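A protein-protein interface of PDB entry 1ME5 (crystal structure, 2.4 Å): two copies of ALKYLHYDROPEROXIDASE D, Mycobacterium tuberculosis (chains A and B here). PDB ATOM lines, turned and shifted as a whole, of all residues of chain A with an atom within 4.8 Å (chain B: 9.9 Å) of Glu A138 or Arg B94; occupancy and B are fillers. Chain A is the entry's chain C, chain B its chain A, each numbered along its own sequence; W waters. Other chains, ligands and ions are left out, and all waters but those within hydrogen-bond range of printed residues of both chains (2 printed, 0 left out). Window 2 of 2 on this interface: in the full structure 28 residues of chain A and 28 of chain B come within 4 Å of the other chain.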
ATOM      1  N   PHE A 122      20.174 -17.788  24.703  1.00  0.00           N
ATOM      2  CA  PHE A 122      20.801 -16.568  25.206  1.00  0.00           C
ATOM      3  C   PHE A 122      19.761 -15.920  26.099  1.00  0.00           C
ATOM      4  O   PHE A 122      19.935 -15.807  27.314  1.00  0.00           O
ATOM      5  CB  PHE A 122      21.123 -15.617  24.054  1.00  0.00           C
ATOM      6  CG  PHE A 122      21.744 -14.322  24.492  1.00  0.00           C
ATOM      7  CD1 PHE A 122      23.045 -14.292  24.990  1.00  0.00           C
ATOM      8  CD2 PHE A 122      21.037 -13.128  24.383  1.00  0.00           C
ATOM      9  CE1 PHE A 122      23.636 -13.083  25.369  1.00  0.00           C
ATOM     10  CE2 PHE A 122      21.612 -11.919  24.757  1.00  0.00           C
ATOM     11  CZ  PHE A 122      22.915 -11.891  25.252  1.00  0.00           C
ATOM     12  N   LEU A 134      25.228 -17.518  29.472  1.00  0.00           N
ATOM     13  CA  LEU A 134      24.961 -16.344  28.659  1.00  0.00           C
ATOM     14  C   LEU A 134      26.145 -16.104  27.717  1.00  0.00           C
ATOM     15  O   LEU A 134      25.967 -15.818  26.533  1.00  0.00           O
ATOM     16  CB  LEU A 134      24.761 -15.111  29.541  1.00  0.00           C
ATOM     17  CG  LEU A 134      24.312 -13.878  28.756  1.00  0.00           C
ATOM     18  CD1 LEU A 134      22.904 -14.141  28.282  1.00  0.00           C
ATOM     19  CD2 LEU A 134      24.362 -12.612  29.606  1.00  0.00           C
ATOM     20  N   VAL A 135      27.348 -16.241  28.266  1.00  0.00           N
ATOM     21  CA  VAL A 135      28.588 -16.038  27.536  1.00  0.00           C
ATOM     22  C   VAL A 135      28.857 -17.034  26.395  1.00  0.00           C
ATOM     23  O   VAL A 135      29.063 -16.619  25.247  1.00  0.00           O
ATOM     24  CB  VAL A 135      29.773 -16.024  28.525  1.00  0.00           C
ATOM     25  CG1 VAL A 135      31.087 -16.176  27.793  1.00  0.00           C
ATOM     26  CG2 VAL A 135      29.755 -14.719  29.287  1.00  0.00           C
ATOM     27  N   ALA A 136      28.847 -18.331  26.700  1.00  0.00           N
ATOM     28  CA  ALA A 136      29.100 -19.349  25.678  1.00  0.00           C
ATOM     29  C   ALA A 136      28.114 -19.301  24.504  1.00  0.00           C
ATOM     30  O   ALA A 136      28.476 -19.643  23.377  1.00  0.00           O
ATOM     31  CB  ALA A 136      29.082 -20.733  26.303  1.00  0.00           C
ATOM     32  N   HIS A 137      26.873 -18.890  24.769  1.00  0.00           N
ATOM     33  CA  HIS A 137      25.854 -18.809  23.728  1.00  0.00           C
ATOM     34  C   HIS A 137      26.072 -17.585  22.871  1.00  0.00           C
ATOM     35  O   HIS A 137      25.730 -17.574  21.692  1.00  0.00           O
ATOM     36  CB  HIS A 137      24.453 -18.769  24.345  1.00  0.00           C
ATOM     37  CG  HIS A 137      23.998 -20.091  24.880  1.00  0.00           C
ATOM     38  ND1 HIS A 137      23.034 -20.208  25.857  1.00  0.00           N
ATOM     39  CD2 HIS A 137      24.407 -21.352  24.602  1.00  0.00           C
ATOM     40  CE1 HIS A 137      22.877 -21.484  26.165  1.00  0.00           C
ATOM     41  NE2 HIS A 137      23.699 -22.198  25.418  1.00  0.00           N
ATOM     42  N   GLU A 138      26.630 -16.542  23.471  1.00  0.00           N
ATOM     43  CA  GLU A 138      26.919 -15.336  22.718  1.00  0.00           C
ATOM     44  C   GLU A 138      28.045 -15.762  21.774  1.00  0.00           C
ATOM     45  O   GLU A 138      28.112 -15.332  20.621  1.00  0.00           O
ATOM     46  CB  GLU A 138      27.390 -14.231  23.663  1.00  0.00           C
ATOM     47  CG  GLU A 138      27.517 -12.863  23.015  1.00  0.00           C
ATOM     48  CD  GLU A 138      28.675 -12.786  22.053  1.00  0.00           C
ATOM     49  OE1 GLU A 138      29.824 -12.854  22.512  1.00  0.00           O
ATOM     50  OE2 GLU A 138      28.438 -12.665  20.835  1.00  0.00           O
ATOM     51  N   HIS A 139      28.907 -16.640  22.277  1.00  0.00           N
ATOM     52  CA  HIS A 139      30.025 -17.168  21.509  1.00  0.00           C
ATOM     53  C   HIS A 139      29.523 -18.073  20.380  1.00  0.00           C
ATOM     54  O   HIS A 139      29.719 -17.753  19.205  1.00  0.00           O
ATOM     55  CB  HIS A 139      30.972 -17.964  22.419  1.00  0.00           C
ATOM     56  CG  HIS A 139      32.158 -18.543  21.704  1.00  0.00           C
ATOM     57  ND1 HIS A 139      33.258 -17.791  21.352  1.00  0.00           N
ATOM     58  CD2 HIS A 139      32.408 -19.801  21.267  1.00  0.00           C
ATOM     59  CE1 HIS A 139      34.135 -18.560  20.731  1.00  0.00           C
ATOM     60  NE2 HIS A 139      33.644 -19.784  20.667  1.00  0.00           N
ATOM     61  N   THR A 140      28.884 -19.193  20.737  1.00  0.00           N
ATOM     62  CA  THR A 140      28.354 -20.144  19.747  1.00  0.00           C
ATOM     63  C   THR A 140      27.564 -19.425  18.673  1.00  0.00           C
ATOM     64  O   THR A 140      27.462 -19.886  17.534  1.00  0.00           O
ATOM     65  CB  THR A 140      27.429 -21.195  20.382  1.00  0.00           C
ATOM     66  OG1 THR A 140      28.151 -21.960  21.361  1.00  0.00           O
ATOM     67  CG2 THR A 140      26.901 -22.146  19.305  1.00  0.00           C
ATOM     68  N   LEU A 141      27.000 -18.288  19.053  1.00  0.00           N
ATOM     69  CA  LEU A 141      26.238 -17.470  18.136  1.00  0.00           C
ATOM     70  C   LEU A 141      27.218 -16.695  17.279  1.00  0.00           C
ATOM     71  O   LEU A 141      27.365 -16.974  16.091  1.00  0.00           O
ATOM     72  CB  LEU A 141      25.347 -16.495  18.908  1.00  0.00           C
ATOM     73  CG  LEU A 141      23.970 -16.992  19.355  1.00  0.00           C
ATOM     74  CD1 LEU A 141      23.484 -16.185  20.554  1.00  0.00           C
ATOM     75  CD2 LEU A 141      22.998 -16.872  18.201  1.00  0.00           C
ATOM     76  N   ARG A 142      27.895 -15.733  17.902  1.00  0.00           N
ATOM     77  CA  ARG A 142      28.856 -14.870  17.221  1.00  0.00           C
ATOM     78  C   ARG A 142      29.609 -15.619  16.131  1.00  0.00           C
ATOM     79  O   ARG A 142      29.882 -15.073  15.062  1.00  0.00           O
ATOM     80  CB  ARG A 142      29.843 -14.291  18.237  1.00  0.00           C
ATOM     81  CG  ARG A 142      30.244 -12.843  17.967  1.00  0.00           C
ATOM     82  CD  ARG A 142      29.062 -11.889  18.140  1.00  0.00           C
ATOM     83  NE  ARG A 142      29.324 -10.571  17.564  1.00  0.00           N
ATOM     84  CZ  ARG A 142      29.540 -10.355  16.267  1.00  0.00           C
ATOM     85  NH1 ARG A 142      29.771  -9.126  15.822  1.00  0.00           N
ATOM     86  NH2 ARG A 142      29.522 -11.368  15.410  1.00  0.00           N
ATOM     87  N   ARG A 148      25.906  -8.341  16.125  1.00  0.00           N
ATOM     88  CA  ARG A 148      26.064  -7.958  17.519  1.00  0.00           C
ATOM     89  C   ARG A 148      24.759  -7.238  17.852  1.00  0.00           C
ATOM     90  O   ARG A 148      24.348  -7.153  19.015  1.00  0.00           O
ATOM     91  CB  ARG A 148      27.277  -7.026  17.650  1.00  0.00           C
ATOM     92  CG  ARG A 148      27.612  -6.531  19.053  1.00  0.00           C
ATOM     93  CD  ARG A 148      29.028  -5.930  19.091  1.00  0.00           C
ATOM     94  NE  ARG A 148      29.301  -5.208  20.329  1.00  0.00           N
ATOM     95  CZ  ARG A 148      29.115  -3.898  20.492  1.00  0.00           C
ATOM     96  NH1 ARG A 148      28.662  -3.161  19.485  1.00  0.00           N
ATOM     97  NH2 ARG A 148      29.370  -3.325  21.666  1.00  0.00           N
ATOM     98  N   ILE A 151      21.894 -10.040  18.625  1.00  0.00           N
ATOM     99  CA  ILE A 151      22.098 -10.625  19.940  1.00  0.00           C
ATOM    100  C   ILE A 151      21.691  -9.686  21.066  1.00  0.00           C
ATOM    101  O   ILE A 151      21.159 -10.120  22.090  1.00  0.00           O
ATOM    102  CB  ILE A 151      23.560 -11.018  20.127  1.00  0.00           C
ATOM    103  CG1 ILE A 151      23.890 -12.167  19.177  1.00  0.00           C
ATOM    104  CG2 ILE A 151      23.822 -11.387  21.586  1.00  0.00           C
ATOM    105  CD1 ILE A 151      25.318 -12.595  19.208  1.00  0.00           C
ATOM    106  N   GLY B  87      22.688  -8.930  32.311  1.00  0.00           N
ATOM    107  CA  GLY B  87      23.177  -9.619  31.129  1.00  0.00           C
ATOM    108  C   GLY B  87      24.340  -8.901  30.465  1.00  0.00           C
ATOM    109  O   GLY B  87      25.327  -9.530  30.091  1.00  0.00           O
ATOM    110  N   ARG B  88      24.211  -7.584  30.320  1.00  0.00           N
ATOM    111  CA  ARG B  88      25.224  -6.749  29.702  1.00  0.00           C
ATOM    112  C   ARG B  88      26.519  -6.779  30.509  1.00  0.00           C
ATOM    113  O   ARG B  88      27.611  -6.693  29.944  1.00  0.00           O
ATOM    114  CB  ARG B  88      24.710  -5.306  29.572  1.00  0.00           C
ATOM    115  CG  ARG B  88      25.070  -4.643  28.244  1.00  0.00           C
ATOM    116  CD  ARG B  88      24.531  -3.225  28.137  1.00  0.00           C
ATOM    117  NE  ARG B  88      24.914  -2.415  29.284  1.00  0.00           N
ATOM    118  CZ  ARG B  88      24.713  -1.106  29.380  1.00  0.00           C
ATOM    119  NH1 ARG B  88      24.132  -0.450  28.381  1.00  0.00           N
ATOM    120  NH2 ARG B  88      25.077  -0.459  30.483  1.00  0.00           N
ATOM    121  N   GLY B  89      26.400  -6.908  31.827  1.00  0.00           N
ATOM    122  CA  GLY B  89      27.578  -6.971  32.673  1.00  0.00           C
ATOM    123  C   GLY B  89      28.274  -8.309  32.530  1.00  0.00           C
ATOM    124  O   GLY B  89      29.487  -8.414  32.706  1.00  0.00           O
ATOM    125  N   PHE B  90      27.485  -9.333  32.215  1.00  0.00           N
ATOM    126  CA  PHE B  90      27.969 -10.698  32.023  1.00  0.00           C
ATOM    127  C   PHE B  90      28.802 -10.758  30.742  1.00  0.00           C
ATOM    128  O   PHE B  90      29.713 -11.566  30.612  1.00  0.00           O
ATOM    129  CB  PHE B  90      26.784 -11.673  31.878  1.00  0.00           C
ATOM    130  CG  PHE B  90      26.130 -12.080  33.186  1.00  0.00           C
ATOM    131  CD1 PHE B  90      26.726 -11.797  34.413  1.00  0.00           C
ATOM    132  CD2 PHE B  90      24.953 -12.831  33.171  1.00  0.00           C
ATOM    133  CE1 PHE B  90      26.168 -12.256  35.606  1.00  0.00           C
ATOM    134  CE2 PHE B  90      24.374 -13.306  34.362  1.00  0.00           C
ATOM    135  CZ  PHE B  90      24.982 -13.021  35.585  1.00  0.00           C
ATOM    136  N   LEU B  91      28.451  -9.897  29.794  1.00  0.00           N
ATOM    137  CA  LEU B  91      29.114  -9.806  28.501  1.00  0.00           C
ATOM    138  C   LEU B  91      30.404  -9.004  28.582  1.00  0.00           C
ATOM    139  O   LEU B  91      31.082  -8.813  27.574  1.00  0.00           O
ATOM    140  CB  LEU B  91      28.170  -9.151  27.498  1.00  0.00           C
ATOM    141  CG  LEU B  91      26.959 -10.009  27.150  1.00  0.00           C
ATOM    142  CD1 LEU B  91      26.083  -9.298  26.128  1.00  0.00           C
ATOM    143  CD2 LEU B  91      27.452 -11.339  26.625  1.00  0.00           C
ATOM    144  N   GLU B  92      30.712  -8.536  29.791  1.00  0.00           N
ATOM    145  CA  GLU B  92      31.907  -7.749  30.088  1.00  0.00           C
ATOM    146  C   GLU B  92      32.019  -6.443  29.299  1.00  0.00           C
ATOM    147  O   GLU B  92      32.987  -6.228  28.569  1.00  0.00           O
ATOM    148  CB  GLU B  92      33.143  -8.608  29.865  1.00  0.00           C
ATOM    149  CG  GLU B  92      33.069  -9.941  30.574  1.00  0.00           C
ATOM    150  CD  GLU B  92      34.274 -10.817  30.288  1.00  0.00           C
ATOM    151  OE1 GLU B  92      35.384 -10.481  30.756  1.00  0.00           O
ATOM    152  OE2 GLU B  92      34.112 -11.838  29.585  1.00  0.00           O
ATOM    153  N   GLY B  93      31.024  -5.575  29.451  1.00  0.00           N
ATOM    154  CA  GLY B  93      31.034  -4.299  28.759  1.00  0.00           C
ATOM    155  C   GLY B  93      31.202  -4.341  27.246  1.00  0.00           C
ATOM    156  O   GLY B  93      31.135  -3.296  26.591  1.00  0.00           O
ATOM    157  N   ARG B  94      31.414  -5.532  26.684  1.00  0.00           N
ATOM    158  CA  ARG B  94      31.587  -5.680  25.240  1.00  0.00           C
ATOM    159  C   ARG B  94      30.412  -5.102  24.462  1.00  0.00           C
ATOM    160  O   ARG B  94      30.440  -5.025  23.237  1.00  0.00           O
ATOM    161  CB  ARG B  94      31.738  -7.147  24.875  1.00  0.00           C
ATOM    162  CG  ARG B  94      33.006  -7.788  25.366  1.00  0.00           C
ATOM    163  CD  ARG B  94      33.140  -9.153  24.737  1.00  0.00           C
ATOM    164  NE  ARG B  94      32.005 -10.010  25.061  1.00  0.00           N
ATOM    165  CZ  ARG B  94      31.672 -11.101  24.377  1.00  0.00           C
ATOM    166  NH1 ARG B  94      32.386 -11.468  23.319  1.00  0.00           N
ATOM    167  NH2 ARG B  94      30.637 -11.839  24.761  1.00  0.00           N
ATOM    168  N   TYR B  95      29.376  -4.705  25.188  1.00  0.00           N
ATOM    169  CA  TYR B  95      28.177  -4.134  24.598  1.00  0.00           C
ATOM    170  C   TYR B  95      27.805  -2.870  25.362  1.00  0.00           C
ATOM    171  O   TYR B  95      26.830  -2.213  25.026  1.00  0.00           O
ATOM    172  CB  TYR B  95      27.003  -5.113  24.719  1.00  0.00           C
ATOM    173  CG  TYR B  95      26.998  -6.306  23.794  1.00  0.00           C
ATOM    174  CD1 TYR B  95      27.861  -7.382  23.995  1.00  0.00           C
ATOM    175  CD2 TYR B  95      26.094  -6.375  22.733  1.00  0.00           C
ATOM    176  CE1 TYR B  95      27.814  -8.515  23.152  1.00  0.00           C
ATOM    177  CE2 TYR B  95      26.046  -7.490  21.888  1.00  0.00           C
ATOM    178  CZ  TYR B  95      26.901  -8.554  22.103  1.00  0.00           C
ATOM    179  OH  TYR B  95      26.839  -9.656  21.283  1.00  0.00           O
ATOM    180  N   ASP B  96      28.581  -2.544  26.395  1.00  0.00           N
ATOM    181  CA  ASP B  96      28.301  -1.392  27.252  1.00  0.00           C
ATOM    182  C   ASP B  96      27.881  -0.102  26.550  1.00  0.00           C
ATOM    183  O   ASP B  96      27.437   0.850  27.199  1.00  0.00           O
ATOM    184  CB  ASP B  96      29.476  -1.138  28.210  1.00  0.00           C
ATOM    185  CG  ASP B  96      29.191  -1.637  29.635  1.00  0.00           C
ATOM    186  OD1 ASP B  96      28.746  -2.801  29.789  1.00  0.00           O
ATOM    187  OD2 ASP B  96      29.410  -0.867  30.603  1.00  0.00           O
ATOM    188  N   ASP B  97      28.022  -0.050  25.232  1.00  0.00           N
ATOM    189  CA  ASP B  97      27.562   1.124  24.513  1.00  0.00           C
ATOM    190  C   ASP B  97      27.112   0.780  23.101  1.00  0.00           C
ATOM    191  O   ASP B  97      27.710   1.185  22.100  1.00  0.00           O
ATOM    192  CB  ASP B  97      28.616   2.226  24.501  1.00  0.00           C
ATOM    193  CG  ASP B  97      27.996   3.605  24.683  1.00  0.00           C
ATOM    194  OD1 ASP B  97      27.211   4.031  23.802  1.00  0.00           O
ATOM    195  OD2 ASP B  97      28.277   4.252  25.716  1.00  0.00           O
ATOM    196  N   LEU B  98      26.034   0.007  23.060  1.00  0.00           N
ATOM    197  CA  LEU B  98      25.413  -0.424  21.825  1.00  0.00           C
ATOM    198  C   LEU B  98      24.052   0.261  21.791  1.00  0.00           C
ATOM    199  O   LEU B  98      23.349   0.211  20.787  1.00  0.00           O
ATOM    200  CB  LEU B  98      25.247  -1.936  21.835  1.00  0.00           C
ATOM    201  CG  LEU B  98      24.781  -2.577  20.539  1.00  0.00           C
ATOM    202  CD1 LEU B  98      25.701  -2.161  19.392  1.00  0.00           C
ATOM    203  CD2 LEU B  98      24.779  -4.079  20.709  1.00  0.00           C
ATOM    204  N   ARG B  99      23.701   0.899  22.909  1.00  0.00           N
ATOM    205  CA  ARG B  99      22.443   1.628  23.067  1.00  0.00           C
ATOM    206  C   ARG B  99      21.231   0.750  23.399  1.00  0.00           C
ATOM    207  O   ARG B  99      20.646   0.110  22.518  1.00  0.00           O
ATOM    208  CB  ARG B  99      22.137   2.457  21.817  1.00  0.00           C
ATOM    209  CG  ARG B  99      20.875   3.289  21.934  1.00  0.00           C
ATOM    210  CD  ARG B  99      20.772   4.293  20.805  1.00  0.00           C
ATOM    211  NE  ARG B  99      20.435   3.676  19.524  1.00  0.00           N
ATOM    212  CZ  ARG B  99      20.535   4.296  18.351  1.00  0.00           C
ATOM    213  NH1 ARG B  99      20.968   5.551  18.296  1.00  0.00           N
ATOM    214  NH2 ARG B  99      20.193   3.668  17.236  1.00  0.00           N
HETATM  215  O   HOH W   1      30.648 -14.262  24.448  1.00  0.00           O
HETATM  216  O   HOH W   2      29.307  -0.960  22.532  1.00  0.00           O
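No position is printed for both chains. Of the 10 pairs that touch across the chains among the printed residues, none has its exchanged pair printed and touching as well.
O of Gly B87 touches CD2 of Leu A134, 3.3 Å away. Leu A134 touches Phe B90. Val A135 touches Phe B90 (CG2 to O, 3.4 Å). CD2 of Leu B91 touches CG of Glu A138, 3.9 Å away. CA of Tyr B95 touches NH2 of Arg A148, 3.3 Å away. Leu B98 touches Arg A148. Ile A151 touches Tyr B95.
The side-chain hydroxyl (OH) of Tyr B95 is in hydrogen-bond range of the side-chain carboxylate (OE2) of Glu A138. The guanidinium group (NH2) of Arg A148 lies within hydrogen-bond range of the backbone carbonyl oxygen (O) of Arg B94, 2.6 Å away. NH2 of Arg B94 is in salt-bridge range of OE1 of Glu A138 (2.6 Å).
Phe A122 touches none of the printed residues of chain B. Val A135 touches just one residue of chain B: Phe B90 (3.4 Å). Glu A138 touches three residues of chain B. Printed residues of chain A within 4 Å of Gly B87: Leu A134 (3.3 Å). Of the printed residues of chain A, Phe B90 touches Leu A134 and Val A135. Printed residues of chain A within 4 Å of Leu B91: Glu A138. Arg B94 touches two residues of chain A. Of the printed residues of chain A, Leu B98 touches Arg A148.
Of the 13 printed residues of chain B, 6 touch a printed residue of chain A. Hydrophobic or aromatic side chains of chain B within 4 Å of the printed part of chain A: Phe B90, Leu B91, Tyr B95 and Leu B98. Along chain B the printed residues that touch a printed residue of chain A span positions 87 to 98. Hydrophobic or aromatic side chains of chain A within 4 Å of the printed part of chain B: Leu A134, Val A135 and Ile A151. Among the printed residues, 10 pairs touch across the chains.
OE2 of Glu A138 is in salt-bridge range of NE of Arg A142 (3.98 Å). The backbone carbonyl oxygen (O) of Leu B91 sits at hydrogen-bond distance from the guanidinium group (NE) of Arg B94.
Water W1 lies within hydrogen-bond range of the guanidinium group (NH2) of Arg B94 (2.4 Å), the side-chain carboxylate (OE1) of Glu A138 (2.5 Å) and the backbone carbonyl oxygen (O) of Val A135 (3.0 Å). Water W2 lies within hydrogen-bond range of the guanidinium group (NH2) of Arg A148, the backbone carbonyl oxygen (O) of Asp B97 and the backbone NH (N) of Leu B98.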
